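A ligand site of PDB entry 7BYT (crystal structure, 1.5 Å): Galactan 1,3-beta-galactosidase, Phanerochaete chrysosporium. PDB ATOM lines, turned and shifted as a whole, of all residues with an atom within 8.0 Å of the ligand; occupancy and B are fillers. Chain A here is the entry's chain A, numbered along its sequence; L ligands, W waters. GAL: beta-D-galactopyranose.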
ATOM      1  N   SER A 317     -18.026   6.946  16.502  1.00  0.00           N
ATOM      2  CA  SER A 317     -17.474   5.598  16.458  1.00  0.00           C
ATOM      3  C   SER A 317     -16.574   5.347  15.242  1.00  0.00           C
ATOM      4  O   SER A 317     -16.296   4.194  14.924  1.00  0.00           O
ATOM      5  CB  SER A 317     -18.600   4.572  16.499  1.00  0.00           C
ATOM      6  OG  SER A 317     -19.711   5.008  15.751  1.00  0.00           O
ATOM      7  N   SER A 318     -16.143   6.393  14.544  1.00  0.00           N
ATOM      8  CA  SER A 318     -15.260   6.154  13.408  1.00  0.00           C
ATOM      9  C   SER A 318     -13.856   5.769  13.875  1.00  0.00           C
ATOM     10  O   SER A 318     -13.436   6.064  14.997  1.00  0.00           O
ATOM     11  CB  SER A 318     -15.205   7.391  12.513  1.00  0.00           C
ATOM     12  OG  SER A 318     -14.775   8.527  13.247  1.00  0.00           O
ATOM     13  N   THR A 319     -13.122   5.094  12.989  1.00  0.00           N
ATOM     14  CA  THR A 319     -11.827   4.507  13.343  1.00  0.00           C
ATOM     15  C   THR A 319     -10.788   4.877  12.302  1.00  0.00           C
ATOM     16  O   THR A 319     -11.098   5.421  11.234  1.00  0.00           O
ATOM     17  CB  THR A 319     -11.912   2.984  13.382  1.00  0.00           C
ATOM     18  OG1 THR A 319     -12.284   2.510  12.080  1.00  0.00           O
ATOM     19  CG2 THR A 319     -12.958   2.508  14.391  1.00  0.00           C
ATOM     20  N   LEU A 321      -8.166   3.149   9.796  1.00  0.00           N
ATOM     21  CA  LEU A 321      -7.792   1.926   9.092  1.00  0.00           C
ATOM     22  C   LEU A 321      -6.412   2.095   8.490  1.00  0.00           C
ATOM     23  O   LEU A 321      -6.040   3.192   8.047  1.00  0.00           O
ATOM     24  CB  LEU A 321      -8.763   1.656   7.934  1.00  0.00           C
ATOM     25  CG  LEU A 321     -10.237   1.528   8.287  1.00  0.00           C
ATOM     26  CD1 LEU A 321     -11.086   1.320   7.029  1.00  0.00           C
ATOM     27  CD2 LEU A 321     -10.416   0.366   9.244  1.00  0.00           C
ATOM     28  N   PHE A 326      -4.215   2.840   0.424  1.00  0.00           N
ATOM     29  CA  PHE A 326      -4.635   4.179   0.808  1.00  0.00           C
ATOM     30  C   PHE A 326      -3.482   5.148   0.674  1.00  0.00           C
ATOM     31  O   PHE A 326      -2.340   4.820   0.995  1.00  0.00           O
ATOM     32  CB  PHE A 326      -5.072   4.221   2.273  1.00  0.00           C
ATOM     33  CG  PHE A 326      -6.156   3.245   2.627  1.00  0.00           C
ATOM     34  CD1 PHE A 326      -7.294   3.098   1.833  1.00  0.00           C
ATOM     35  CD2 PHE A 326      -6.074   2.513   3.803  1.00  0.00           C
ATOM     36  CE1 PHE A 326      -8.303   2.208   2.193  1.00  0.00           C
ATOM     37  CE2 PHE A 326      -7.078   1.634   4.169  1.00  0.00           C
ATOM     38  CZ  PHE A 326      -8.192   1.473   3.363  1.00  0.00           C
ATOM     39  N   VAL A 332     -10.181   6.494   7.049  1.00  0.00           N
ATOM     40  CA  VAL A 332     -11.120   6.533   8.165  1.00  0.00           C
ATOM     41  C   VAL A 332     -12.212   5.526   7.895  1.00  0.00           C
ATOM     42  O   VAL A 332     -12.864   5.575   6.847  1.00  0.00           O
ATOM     43  CB  VAL A 332     -11.681   7.944   8.390  1.00  0.00           C
ATOM     44  CG1 VAL A 332     -12.739   7.929   9.504  1.00  0.00           C
ATOM     45  CG2 VAL A 332     -10.555   8.911   8.747  1.00  0.00           C
ATOM     46  N   GLY A 333     -12.411   4.607   8.843  1.00  0.00           N
ATOM     47  CA  GLY A 333     -13.407   3.564   8.743  1.00  0.00           C
ATOM     48  C   GLY A 333     -14.548   3.775   9.715  1.00  0.00           C
ATOM     49  O   GLY A 333     -14.561   4.714  10.512  1.00  0.00           O
ATOM     50  N   TYR A 334     -15.516   2.862   9.651  1.00  0.00           N
ATOM     51  CA  TYR A 334     -16.723   2.951  10.481  1.00  0.00           C
ATOM     52  C   TYR A 334     -17.339   4.354  10.438  1.00  0.00           C
ATOM     53  O   TYR A 334     -17.721   4.934  11.455  1.00  0.00           O
ATOM     54  CB  TYR A 334     -16.461   2.414  11.901  1.00  0.00           C
ATOM     55  CG  TYR A 334     -16.367   0.899  11.861  1.00  0.00           C
ATOM     56  CD1 TYR A 334     -15.175   0.269  11.507  1.00  0.00           C
ATOM     57  CD2 TYR A 334     -17.485   0.114  12.084  1.00  0.00           C
ATOM     58  CE1 TYR A 334     -15.102  -1.115  11.428  1.00  0.00           C
ATOM     59  CE2 TYR A 334     -17.412  -1.271  12.006  1.00  0.00           C
ATOM     60  CZ  TYR A 334     -16.217  -1.865  11.680  1.00  0.00           C
ATOM     61  OH  TYR A 334     -16.159  -3.246  11.609  1.00  0.00           O
ATOM     62  N   LEU A 335     -17.411   4.900   9.224  1.00  0.00           N
ATOM     63  CA  LEU A 335     -18.078   6.164   8.983  1.00  0.00           C
ATOM     64  C   LEU A 335     -19.560   5.909   8.743  1.00  0.00           C
ATOM     65  O   LEU A 335     -19.957   4.884   8.195  1.00  0.00           O
ATOM     66  CB  LEU A 335     -17.480   6.876   7.771  1.00  0.00           C
ATOM     67  CG  LEU A 335     -16.150   7.567   8.033  1.00  0.00           C
ATOM     68  CD1 LEU A 335     -15.582   8.057   6.716  1.00  0.00           C
ATOM     69  CD2 LEU A 335     -16.347   8.743   9.010  1.00  0.00           C
ATOM     70  N   GLY A 336     -20.376   6.885   9.147  1.00  0.00           N
ATOM     71  CA  GLY A 336     -21.807   6.653   9.210  1.00  0.00           C
ATOM     72  C   GLY A 336     -22.101   5.777  10.412  1.00  0.00           C
ATOM     73  O   GLY A 336     -21.207   5.341  11.132  1.00  0.00           O
ATOM     74  N   HIS A 337     -23.390   5.511  10.617  1.00  0.00           N
ATOM     75  CA  HIS A 337     -23.834   4.700  11.750  1.00  0.00           C
ATOM     76  C   HIS A 337     -23.191   5.183  13.048  1.00  0.00           C
ATOM     77  O   HIS A 337     -22.673   4.394  13.843  1.00  0.00           O
ATOM     78  CB  HIS A 337     -23.560   3.214  11.500  1.00  0.00           C
ATOM     79  CG  HIS A 337     -24.299   2.299  12.432  1.00  0.00           C
ATOM     80  ND1 HIS A 337     -25.662   2.093  12.327  1.00  0.00           N
ATOM     81  CD2 HIS A 337     -23.866   1.555  13.471  1.00  0.00           C
ATOM     82  CE1 HIS A 337     -26.042   1.246  13.275  1.00  0.00           C
ATOM     83  NE2 HIS A 337     -24.971   0.901  13.979  1.00  0.00           N
ATOM     84  N   ALA A 360     -12.655   3.496  -0.293  1.00  0.00           N
ATOM     85  CA  ALA A 360     -12.721   2.064  -0.577  1.00  0.00           C
ATOM     86  C   ALA A 360     -14.068   1.539  -0.101  1.00  0.00           C
ATOM     87  O   ALA A 360     -14.556   1.932   0.962  1.00  0.00           O
ATOM     88  CB  ALA A 360     -11.597   1.310   0.147  1.00  0.00           C
ATOM     89  N   ASN A 361     -14.656   0.646  -0.884  1.00  0.00           N
ATOM     90  CA  ASN A 361     -15.936   0.023  -0.543  1.00  0.00           C
ATOM     91  C   ASN A 361     -15.867  -1.439  -0.995  1.00  0.00           C
ATOM     92  O   ASN A 361     -16.030  -1.729  -2.185  1.00  0.00           O
ATOM     93  CB  ASN A 361     -17.098   0.756  -1.230  1.00  0.00           C
ATOM     94  CG  ASN A 361     -18.428   0.050  -1.046  1.00  0.00           C
ATOM     95  OD1 ASN A 361     -18.551  -0.896  -0.264  1.00  0.00           O
ATOM     96  ND2 ASN A 361     -19.436   0.516  -1.772  1.00  0.00           N
ATOM     97  N   GLY A 362     -15.633  -2.341  -0.044  1.00  0.00           N
ATOM     98  CA  GLY A 362     -15.503  -3.755  -0.366  1.00  0.00           C
ATOM     99  C   GLY A 362     -16.795  -4.490  -0.637  1.00  0.00           C
ATOM    100  O   GLY A 362     -16.739  -5.649  -1.068  1.00  0.00           O
ATOM    101  N   ASP A 363     -17.944  -3.855  -0.412  1.00  0.00           N
ATOM    102  CA  ASP A 363     -19.205  -4.502  -0.728  1.00  0.00           C
ATOM    103  C   ASP A 363     -19.394  -4.579  -2.245  1.00  0.00           C
ATOM    104  O   ASP A 363     -18.694  -3.916  -3.017  1.00  0.00           O
ATOM    105  CB  ASP A 363     -20.368  -3.731  -0.102  1.00  0.00           C
ATOM    106  CG  ASP A 363     -20.353  -3.765   1.419  1.00  0.00           C
ATOM    107  OD1 ASP A 363     -19.798  -4.720   1.994  1.00  0.00           O
ATOM    108  OD2 ASP A 363     -20.955  -2.852   2.021  1.00  0.00           O
ATOM    109  N   ARG A 367     -22.438   2.065  -1.400  1.00  0.00           N
ATOM    110  CA  ARG A 367     -22.665   2.771  -0.155  1.00  0.00           C
ATOM    111  C   ARG A 367     -22.927   4.240  -0.511  1.00  0.00           C
ATOM    112  O   ARG A 367     -23.077   4.601  -1.676  1.00  0.00           O
ATOM    113  CB  ARG A 367     -21.483   2.572   0.784  1.00  0.00           C
ATOM    114  CG  ARG A 367     -21.309   1.134   1.280  1.00  0.00           C
ATOM    115  CD  ARG A 367     -20.199   1.054   2.312  1.00  0.00           C
ATOM    116  NE  ARG A 367     -19.979  -0.313   2.761  1.00  0.00           N
ATOM    117  CZ  ARG A 367     -19.317  -0.639   3.866  1.00  0.00           C
ATOM    118  NH1 ARG A 367     -18.794   0.305   4.640  1.00  0.00           N
ATOM    119  NH2 ARG A 367     -19.165  -1.913   4.188  1.00  0.00           N
ATOM    120  N   GLY A 388     -12.657  -3.611  -3.540  1.00  0.00           N
ATOM    121  CA  GLY A 388     -11.995  -4.174  -2.376  1.00  0.00           C
ATOM    122  C   GLY A 388     -11.855  -3.189  -1.239  1.00  0.00           C
ATOM    123  O   GLY A 388     -11.869  -1.971  -1.454  1.00  0.00           O
ATOM    124  N   GLY A 389     -11.698  -3.706  -0.027  1.00  0.00           N
ATOM    125  CA  GLY A 389     -11.462  -2.840   1.108  1.00  0.00           C
ATOM    126  C   GLY A 389     -10.146  -2.099   1.039  1.00  0.00           C
ATOM    127  O   GLY A 389      -9.965  -1.108   1.750  1.00  0.00           O
ATOM    128  N   ASN A 390      -9.224  -2.560   0.193  1.00  0.00           N
ATOM    129  CA  ASN A 390      -7.922  -1.924   0.025  1.00  0.00           C
ATOM    130  C   ASN A 390      -7.772  -1.378  -1.392  1.00  0.00           C
ATOM    131  O   ASN A 390      -6.640  -1.136  -1.838  1.00  0.00           O
ATOM    132  CB  ASN A 390      -6.803  -2.928   0.352  1.00  0.00           C
ATOM    133  CG  ASN A 390      -5.467  -2.264   0.692  1.00  0.00           C
ATOM    134  OD1 ASN A 390      -5.410  -1.215   1.351  1.00  0.00           O
ATOM    135  ND2 ASN A 390      -4.375  -2.897   0.272  1.00  0.00           N
ATOM    136  N   ASN A 416     -26.715   3.947   7.837  1.00  0.00           N
ATOM    137  CA  ASN A 416     -25.888   2.964   7.151  1.00  0.00           C
ATOM    138  C   ASN A 416     -24.423   3.372   7.246  1.00  0.00           C
ATOM    139  O   ASN A 416     -24.076   4.537   7.441  1.00  0.00           O
ATOM    140  CB  ASN A 416     -26.296   2.865   5.682  1.00  0.00           C
ATOM    141  CG  ASN A 416     -26.175   4.198   4.940  1.00  0.00           C
ATOM    142  OD1 ASN A 416     -26.759   5.201   5.362  1.00  0.00           O
ATOM    143  ND2 ASN A 416     -25.439   4.216   3.839  1.00  0.00           N
ATOM    144  N   TYR A 417     -23.551   2.373   7.112  1.00  0.00           N
ATOM    145  CA  TYR A 417     -22.125   2.646   7.019  1.00  0.00           C
ATOM    146  C   TYR A 417     -21.783   3.228   5.655  1.00  0.00           C
ATOM    147  O   TYR A 417     -22.189   2.701   4.604  1.00  0.00           O
ATOM    148  CB  TYR A 417     -21.315   1.379   7.258  1.00  0.00           C
ATOM    149  CG  TYR A 417     -21.233   0.971   8.720  1.00  0.00           C
ATOM    150  CD1 TYR A 417     -20.541   1.748   9.633  1.00  0.00           C
ATOM    151  CD2 TYR A 417     -21.868  -0.171   9.171  1.00  0.00           C
ATOM    152  CE1 TYR A 417     -20.468   1.376  10.980  1.00  0.00           C
ATOM    153  CE2 TYR A 417     -21.806  -0.552  10.498  1.00  0.00           C
ATOM    154  CZ  TYR A 417     -21.113   0.235  11.396  1.00  0.00           C
ATOM    155  OH  TYR A 417     -21.052  -0.146  12.724  1.00  0.00           O
ATOM    156  N   ALA A 418     -21.057   4.339   5.669  1.00  0.00           N
ATOM    157  CA  ALA A 418     -20.477   4.911   4.471  1.00  0.00           C
ATOM    158  C   ALA A 418     -19.259   4.087   4.062  1.00  0.00           C
ATOM    159  O   ALA A 418     -18.813   3.186   4.775  1.00  0.00           O
ATOM    160  CB  ALA A 418     -20.049   6.345   4.756  1.00  0.00           C
ATOM    161  N   ALA A 419     -18.711   4.420   2.898  1.00  0.00           N
ATOM    162  CA  ALA A 419     -17.440   3.821   2.530  1.00  0.00           C
ATOM    163  C   ALA A 419     -16.317   4.364   3.401  1.00  0.00           C
ATOM    164  O   ALA A 419     -16.457   5.355   4.115  1.00  0.00           O
ATOM    165  CB  ALA A 419     -17.132   4.075   1.052  1.00  0.00           C
ATOM    166  N   ASP A 420     -15.164   3.697   3.333  1.00  0.00           N
ATOM    167  CA  ASP A 420     -13.993   4.122   4.076  1.00  0.00           C
ATOM    168  C   ASP A 420     -13.303   5.264   3.324  1.00  0.00           C
ATOM    169  O   ASP A 420     -12.975   5.127   2.151  1.00  0.00           O
ATOM    170  CB  ASP A 420     -13.034   2.952   4.225  1.00  0.00           C
ATOM    171  CG  ASP A 420     -13.659   1.784   4.974  1.00  0.00           C
ATOM    172  OD1 ASP A 420     -14.475   2.036   5.892  1.00  0.00           O
ATOM    173  OD2 ASP A 420     -13.316   0.636   4.651  1.00  0.00           O
ATOM    174  N   LEU A 421     -13.081   6.381   4.007  1.00  0.00           N
ATOM    175  CA  LEU A 421     -12.623   7.600   3.335  1.00  0.00           C
ATOM    176  C   LEU A 421     -11.108   7.707   3.447  1.00  0.00           C
ATOM    177  O   LEU A 421     -10.560   7.786   4.558  1.00  0.00           O
ATOM    178  CB  LEU A 421     -13.294   8.830   3.955  1.00  0.00           C
ATOM    179  CG  LEU A 421     -13.109  10.124   3.161  1.00  0.00           C
ATOM    180  CD1 LEU A 421     -13.688  10.045   1.749  1.00  0.00           C
ATOM    181  CD2 LEU A 421     -13.718  11.293   3.946  1.00  0.00           C
HETATM  182  C1  GAL L   1     -16.077  -2.587   6.224  1.00  0.00           C
HETATM  183  C2  GAL L   1     -15.385  -1.241   6.405  1.00  0.00           C
HETATM  184  C3  GAL L   1     -15.585  -0.701   7.836  1.00  0.00           C
HETATM  185  C4  GAL L   1     -17.078  -0.634   8.178  1.00  0.00           C
HETATM  186  C5  GAL L   1     -17.660  -2.016   7.917  1.00  0.00           C
HETATM  187  C6  GAL L   1     -19.159  -2.094   8.102  1.00  0.00           C
HETATM  188  O1  GAL L   1     -15.997  -2.990   4.873  1.00  0.00           O
HETATM  189  O2  GAL L   1     -13.987  -1.383   6.172  1.00  0.00           O
HETATM  190  O3  GAL L   1     -15.023   0.610   7.983  1.00  0.00           O
HETATM  191  O4  GAL L   1     -17.767   0.322   7.333  1.00  0.00           O
HETATM  192  O5  GAL L   1     -17.423  -2.440   6.561  1.00  0.00           O
HETATM  193  O6  GAL L   1     -19.588  -3.466   8.174  1.00  0.00           O
HETATM  194  O   HOH W   1     -12.528  -3.594   4.389  1.00  0.00           O
HETATM  195  O   HOH W   2     -16.973   3.009   6.876  1.00  0.00           O
HETATM  196  O   HOH W   3     -15.372  -5.375   4.466  1.00  0.00           O
HETATM  197  O   HOH W   4     -18.410  -4.719  10.451  1.00  0.00           O
HETATM  198  O   HOH W   5     -12.313  -2.664   8.030  1.00  0.00           O
HETATM  199  O   HOH W   6     -15.025  -1.331   2.679  1.00  0.00           O
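Residues that only touch the ligand: Gly 333 (3.5 Å), Tyr 417 (3.5 Å) and Ala 418 (3.98 Å). Hydrophobic or aromatic side chains that line the ligand: Tyr 334 and Tyr 417. Of the 25 residues printed, 6 come within 4 Å of the ligand.
NE of Arg 367 is in salt-bridge range of OD2 of Asp 363. The backbone carbonyl oxygen of Thr 319 is in hydrogen-bond range of the backbone NH of Gly 333, 2.8 Å away. The backbone carbonyl oxygen (O) of Asp 420 lies within hydrogen-bond range of the backbone NH (N) of Ala 360. N of Ala 418 is in hydrogen-bond range of O of Leu 335 (2.8 Å). The guanidinium group of Arg 367 sits at hydrogen-bond distance from the side-chain amide oxygen of Asn 361. NH1 of Arg 367 sits at hydrogen-bond distance from O of Ala 418 (2.9 Å).
N of Tyr 334 lies within hydrogen-bond range of O3 of the ligand (2.8 Å). The side-chain carboxylate (OD1) of Asp 420 lies within hydrogen-bond range of an oxygen (O3) of the ligand, 2.6 Å away. NH1 of Arg 367 lies within hydrogen-bond range of O4 of the ligand (2.9 Å).
Water W2 lies within hydrogen-bond range of O of Ala 418 (2.8 Å), O4 of the ligand (2.8 Å), OD1 of Asp 420 (2.9 Å), N of Leu 335 (3.0 Å) and N of Tyr 334 (3.1 Å). Water W4 bridges O6 of the ligand (2.9 Å) and OH of Tyr 334 (2.9 Å). Water W6 lies within hydrogen-bond range of an oxygen (O1) of the ligand, the backbone NH (N) of Gly 362 and the side-chain carboxylate (OD2) of Asp 420.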
